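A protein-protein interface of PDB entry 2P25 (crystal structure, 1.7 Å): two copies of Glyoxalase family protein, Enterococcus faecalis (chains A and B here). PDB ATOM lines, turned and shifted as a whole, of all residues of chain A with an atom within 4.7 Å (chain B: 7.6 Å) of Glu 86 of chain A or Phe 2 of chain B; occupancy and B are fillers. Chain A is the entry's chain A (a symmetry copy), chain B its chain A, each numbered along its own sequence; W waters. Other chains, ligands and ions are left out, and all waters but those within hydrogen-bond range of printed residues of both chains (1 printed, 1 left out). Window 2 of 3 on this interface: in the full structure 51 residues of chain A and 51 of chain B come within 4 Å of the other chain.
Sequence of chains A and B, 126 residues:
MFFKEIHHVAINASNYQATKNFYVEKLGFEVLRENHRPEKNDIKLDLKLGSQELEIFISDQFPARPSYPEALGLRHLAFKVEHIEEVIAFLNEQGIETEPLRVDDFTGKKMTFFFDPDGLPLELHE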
ATOM      1  N   LYS A  80      10.998  20.171  23.866  1.00  0.00           N
ATOM      2  CA  LYS A  80      10.836  18.737  23.684  1.00  0.00           C
ATOM      3  C   LYS A  80      10.447  18.486  22.225  1.00  0.00           C
ATOM      4  O   LYS A  80       9.544  19.158  21.696  1.00  0.00           O
ATOM      5  CB  LYS A  80       9.745  18.145  24.599  1.00  0.00           C
ATOM      6  CG  LYS A  80       9.829  16.592  24.652  1.00  0.00           C
ATOM      7  CD  LYS A  80       8.807  15.957  25.581  1.00  0.00           C
ATOM      8  CE  LYS A  80       8.803  14.455  25.374  1.00  0.00           C
ATOM      9  NZ  LYS A  80       9.005  14.146  23.914  1.00  0.00           N
ATOM     10  N   VAL A  81      11.163  17.567  21.584  1.00  0.00           N
ATOM     11  CA  VAL A  81      10.848  17.168  20.201  1.00  0.00           C
ATOM     12  C   VAL A  81      10.599  15.673  20.114  1.00  0.00           C
ATOM     13  O   VAL A  81      11.088  14.879  20.933  1.00  0.00           O
ATOM     14  CB  VAL A  81      11.956  17.611  19.172  1.00  0.00           C
ATOM     15  CG1 VAL A  81      12.140  19.167  19.190  1.00  0.00           C
ATOM     16  CG2 VAL A  81      13.277  16.947  19.478  1.00  0.00           C
ATOM     17  N   HIS A  83      11.058  13.772  17.030  1.00  0.00           N
ATOM     18  CA  HIS A  83      12.154  13.209  16.266  1.00  0.00           C
ATOM     19  C   HIS A  83      13.082  14.346  15.893  1.00  0.00           C
ATOM     20  O   HIS A  83      12.748  15.228  15.084  1.00  0.00           O
ATOM     21  CB  HIS A  83      11.664  12.407  15.050  1.00  0.00           C
ATOM     22  CG  HIS A  83      12.597  11.303  14.654  1.00  0.00           C
ATOM     23  ND1 HIS A  83      13.406  11.371  13.539  1.00  0.00           N
ATOM     24  CD2 HIS A  83      12.875  10.119  15.249  1.00  0.00           C
ATOM     25  CE1 HIS A  83      14.130  10.270  13.458  1.00  0.00           C
ATOM     26  NE2 HIS A  83      13.824   9.491  14.481  1.00  0.00           N
ATOM     27  N   ILE A  84      14.231  14.345  16.553  1.00  0.00           N
ATOM     28  CA  ILE A  84      15.158  15.489  16.529  1.00  0.00           C
ATOM     29  C   ILE A  84      15.755  15.816  15.148  1.00  0.00           C
ATOM     30  O   ILE A  84      15.919  16.979  14.803  1.00  0.00           O
ATOM     31  CB  ILE A  84      16.244  15.323  17.603  1.00  0.00           C
ATOM     32  CG1 ILE A  84      16.934  16.660  17.887  1.00  0.00           C
ATOM     33  CG2 ILE A  84      17.229  14.193  17.226  1.00  0.00           C
ATOM     34  CD1 ILE A  84      17.654  16.653  19.226  1.00  0.00           C
ATOM     35  N   GLU A  85      16.003  14.790  14.339  1.00  0.00           N
ATOM     36  CA  GLU A  85      16.618  14.970  13.023  1.00  0.00           C
ATOM     37  C   GLU A  85      15.797  15.879  12.121  1.00  0.00           C
ATOM     38  O   GLU A  85      16.358  16.732  11.415  1.00  0.00           O
ATOM     39  CB  GLU A  85      16.866  13.591  12.360  1.00  0.00           C
ATOM     40  CG  GLU A  85      17.994  12.816  13.069  1.00  0.00           C
ATOM     41  CD  GLU A  85      17.520  11.925  14.229  1.00  0.00           C
ATOM     42  OE1 GLU A  85      16.312  11.895  14.555  1.00  0.00           O
ATOM     43  OE2 GLU A  85      18.384  11.254  14.846  1.00  0.00           O
ATOM     44  N   GLU A  86      14.471  15.718  12.148  1.00  0.00           N
ATOM     45  CA  GLU A  86      13.608  16.559  11.311  1.00  0.00           C
ATOM     46  C   GLU A  86      13.593  18.011  11.763  1.00  0.00           C
ATOM     47  O   GLU A  86      13.529  18.925  10.932  1.00  0.00           O
ATOM     48  CB  GLU A  86      12.185  16.012  11.189  1.00  0.00           C
ATOM     49  CG  GLU A  86      11.324  16.079  12.427  1.00  0.00           C
ATOM     50  CD  GLU A  86       9.893  15.636  12.161  1.00  0.00           C
ATOM     51  OE1 GLU A  86       9.639  15.125  11.051  1.00  0.00           O
ATOM     52  OE2 GLU A  86       9.031  15.767  13.062  1.00  0.00           O
ATOM     53  N   VAL A  87      13.651  18.216  13.078  1.00  0.00           N
ATOM     54  CA  VAL A  87      13.676  19.587  13.610  1.00  0.00           C
ATOM     55  C   VAL A  87      15.006  20.258  13.237  1.00  0.00           C
ATOM     56  O   VAL A  87      15.036  21.421  12.800  1.00  0.00           O
ATOM     57  CB  VAL A  87      13.363  19.638  15.123  1.00  0.00           C
ATOM     58  CG1 VAL A  87      13.228  21.095  15.574  1.00  0.00           C
ATOM     59  CG2 VAL A  87      12.052  18.875  15.415  1.00  0.00           C
ATOM     60  N   ILE A  88      16.107  19.531  13.408  1.00  0.00           N
ATOM     61  CA  ILE A  88      17.413  20.027  12.955  1.00  0.00           C
ATOM     62  C   ILE A  88      17.385  20.389  11.466  1.00  0.00           C
ATOM     63  O   ILE A  88      17.843  21.470  11.064  1.00  0.00           O
ATOM     64  CB  ILE A  88      18.523  19.008  13.292  1.00  0.00           C
ATOM     65  CG1 ILE A  88      18.777  18.985  14.804  1.00  0.00           C
ATOM     66  CG2 ILE A  88      19.821  19.324  12.535  1.00  0.00           C
ATOM     67  CD1 ILE A  88      19.571  17.759  15.243  1.00  0.00           C
ATOM     68  N   ALA A  89      16.834  19.495  10.633  1.00  0.00           N
ATOM     69  CA  ALA A  89      16.777  19.748   9.205  1.00  0.00           C
ATOM     70  C   ALA A  89      15.993  21.030   8.935  1.00  0.00           C
ATOM     71  O   ALA A  89      16.438  21.880   8.145  1.00  0.00           O
ATOM     72  CB  ALA A  89      16.144  18.555   8.467  1.00  0.00           C
ATOM     73  N   PHE A  90      14.829  21.161   9.580  1.00  0.00           N
ATOM     74  CA  PHE A  90      13.996  22.364   9.463  1.00  0.00           C
ATOM     75  C   PHE A  90      14.778  23.636   9.809  1.00  0.00           C
ATOM     76  O   PHE A  90      14.777  24.606   9.045  1.00  0.00           O
ATOM     77  CB  PHE A  90      12.711  22.256  10.325  1.00  0.00           C
ATOM     78  CG  PHE A  90      11.972  23.566  10.460  1.00  0.00           C
ATOM     79  CD1 PHE A  90      11.100  23.993   9.466  1.00  0.00           C
ATOM     80  CD2 PHE A  90      12.193  24.388  11.570  1.00  0.00           C
ATOM     81  CE1 PHE A  90      10.427  25.217   9.591  1.00  0.00           C
ATOM     82  CE2 PHE A  90      11.534  25.607  11.702  1.00  0.00           C
ATOM     83  CZ  PHE A  90      10.660  26.024  10.715  1.00  0.00           C
ATOM     84  N   MET B   1       4.483  23.009  14.349  1.00  0.00           N
ATOM     85  CA  MET B   1       4.353  22.808  15.821  1.00  0.00           C
ATOM     86  C   MET B   1       5.598  22.201  16.505  1.00  0.00           C
ATOM     87  O   MET B   1       5.511  21.651  17.610  1.00  0.00           O
ATOM     88  CB  MET B   1       3.089  22.004  16.132  1.00  0.00           C
ATOM     89  CG  MET B   1       1.791  22.766  15.814  1.00  0.00           C
ATOM     90  SD  MET B   1       1.395  24.218  17.092  1.00  0.00           S
ATOM     91  CE  MET B   1       0.025  23.322  18.184  1.00  0.00           C
ATOM     92  N   PHE B   2       6.760  22.334  15.871  1.00  0.00           N
ATOM     93  CA  PHE B   2       8.004  21.818  16.455  1.00  0.00           C
ATOM     94  C   PHE B   2       8.407  22.413  17.805  1.00  0.00           C
ATOM     95  O   PHE B   2       9.117  21.768  18.592  1.00  0.00           O
ATOM     96  CB  PHE B   2       9.162  22.031  15.493  1.00  0.00           C
ATOM     97  CG  PHE B   2       9.163  21.090  14.328  1.00  0.00           C
ATOM     98  CD1 PHE B   2       8.538  19.853  14.421  1.00  0.00           C
ATOM     99  CD2 PHE B   2       9.830  21.428  13.155  1.00  0.00           C
ATOM    100  CE1 PHE B   2       8.551  18.969  13.343  1.00  0.00           C
ATOM    101  CE2 PHE B   2       9.868  20.545  12.073  1.00  0.00           C
ATOM    102  CZ  PHE B   2       9.224  19.316  12.166  1.00  0.00           C
ATOM    103  N   PHE B   3       7.984  23.644  18.062  1.00  0.00           N
ATOM    104  CA  PHE B   3       8.520  24.389  19.210  1.00  0.00           C
ATOM    105  C   PHE B   3       7.449  24.729  20.220  1.00  0.00           C
ATOM    106  O   PHE B   3       7.601  25.666  21.006  1.00  0.00           O
ATOM    107  CB  PHE B   3       9.242  25.644  18.714  1.00  0.00           C
ATOM    108  CG  PHE B   3      10.317  25.343  17.727  1.00  0.00           C
ATOM    109  CD1 PHE B   3      11.563  24.918  18.161  1.00  0.00           C
ATOM    110  CD2 PHE B   3      10.079  25.444  16.364  1.00  0.00           C
ATOM    111  CE1 PHE B   3      12.553  24.624  17.265  1.00  0.00           C
ATOM    112  CE2 PHE B   3      11.069  25.143  15.449  1.00  0.00           C
ATOM    113  CZ  PHE B   3      12.304  24.709  15.902  1.00  0.00           C
ATOM    114  N   LYS B   4       6.386  23.940  20.214  1.00  0.00           N
ATOM    115  CA  LYS B   4       5.215  24.215  21.035  1.00  0.00           C
ATOM    116  C   LYS B   4       5.362  23.834  22.511  1.00  0.00           C
ATOM    117  O   LYS B   4       4.590  24.340  23.339  1.00  0.00           O
ATOM    118  CB  LYS B   4       3.964  23.533  20.450  1.00  0.00           C
ATOM    119  CG  LYS B   4       3.940  22.003  20.600  1.00  0.00           C
ATOM    120  CD  LYS B   4       2.601  21.401  20.196  1.00  0.00           C
ATOM    121  CE  LYS B   4       2.700  19.886  19.985  1.00  0.00           C
ATOM    122  NZ  LYS B   4       3.204  19.541  18.621  1.00  0.00           N
ATOM    123  N   GLU B   5       6.315  22.942  22.825  1.00  0.00           N
ATOM    124  CA  GLU B   5       6.406  22.311  24.152  1.00  0.00           C
ATOM    125  C   GLU B   5       7.784  22.508  24.788  1.00  0.00           C
ATOM    126  O   GLU B   5       8.798  22.130  24.205  1.00  0.00           O
ATOM    127  CB  GLU B   5       6.070  20.810  24.066  1.00  0.00           C
ATOM    128  CG  GLU B   5       6.034  20.090  25.408  1.00  0.00           C
ATOM    129  CD  GLU B   5       5.770  18.583  25.291  1.00  0.00           C
ATOM    130  OE1 GLU B   5       5.420  18.094  24.182  1.00  0.00           O
ATOM    131  OE2 GLU B   5       5.919  17.886  26.326  1.00  0.00           O
HETATM  132  O   HOH W   1       6.751  17.411  21.236  1.00  0.00           O
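The backbone carbonyl oxygen (O) of Glu 5 of chain B lies within hydrogen-bond range of the backbone NH (N) of Lys 80 of chain A (3.0 Å).
Among the printed residues, merely in contact across the chains: Glu 86 of chain A with Phe 2 of chain B (3.2 Å), Val 87 of chain A with Phe 3 of chain B (3.7 Å), Phe 90 of chain A with Phe 2 of chain B (3.8 Å), Val 87 of chain A with Phe 2 of chain B (3.8 Å) and Phe 90 of chain A with Phe 3 of chain B (3.8 Å).
Of chain B, only Phe 2 (3.2 Å) comes within 4 Å of Glu 86 of chain A.
Of chain A, only Glu 86 (3.2 Å), Val 87 (3.8 Å) and Phe 90 (3.8 Å) come within 4 Å of Phe 2 of chain B.
Of the printed residues of chain A, Glu 5 of chain B touches Lys 80 (3.0 Å).
Of the printed residues of chain A, Phe 3 of chain B touches Val 87 (3.7 Å) and Phe 90 (3.8 Å).
Of the printed residues of chain B, Val 87 of chain A touches Phe 2 and Phe 3.
Of the printed residues of chain B, Phe 90 of chain A touches Phe 2 (3.8 Å) and Phe 3 (3.8 Å).
Val 81 of chain A touches none of the printed residues of chain B.
The nearest residue of chain A that does not touch Phe 2 of chain B is Val 81 of chain A (4.03 Å).
Of the 10 printed residues of chain A, 4 touch a printed residue of chain B.
Along chain A the printed residues that touch a printed residue of chain B span positions 80 to 90.
Of the 5 printed residues of chain B, 3 touch a printed residue of chain A.
Hydrophobic or aromatic side chains of chain B within 4 Å of the printed part of chain A: Phe 2 and Phe 3.
Among the printed residues, 6 pairs touch across the chains.
Among the printed residues, no Asp or Glu carboxylate lies within 4 Å of a Lys or Arg side-chain nitrogen of the other chain.
No position is printed for both chains.
Water W1 bridges the side-chain carboxylate of Glu 5 of chain B (3.3 Å) and the backbone carbonyl oxygen of Lys 80 of chain A (3.3 Å).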
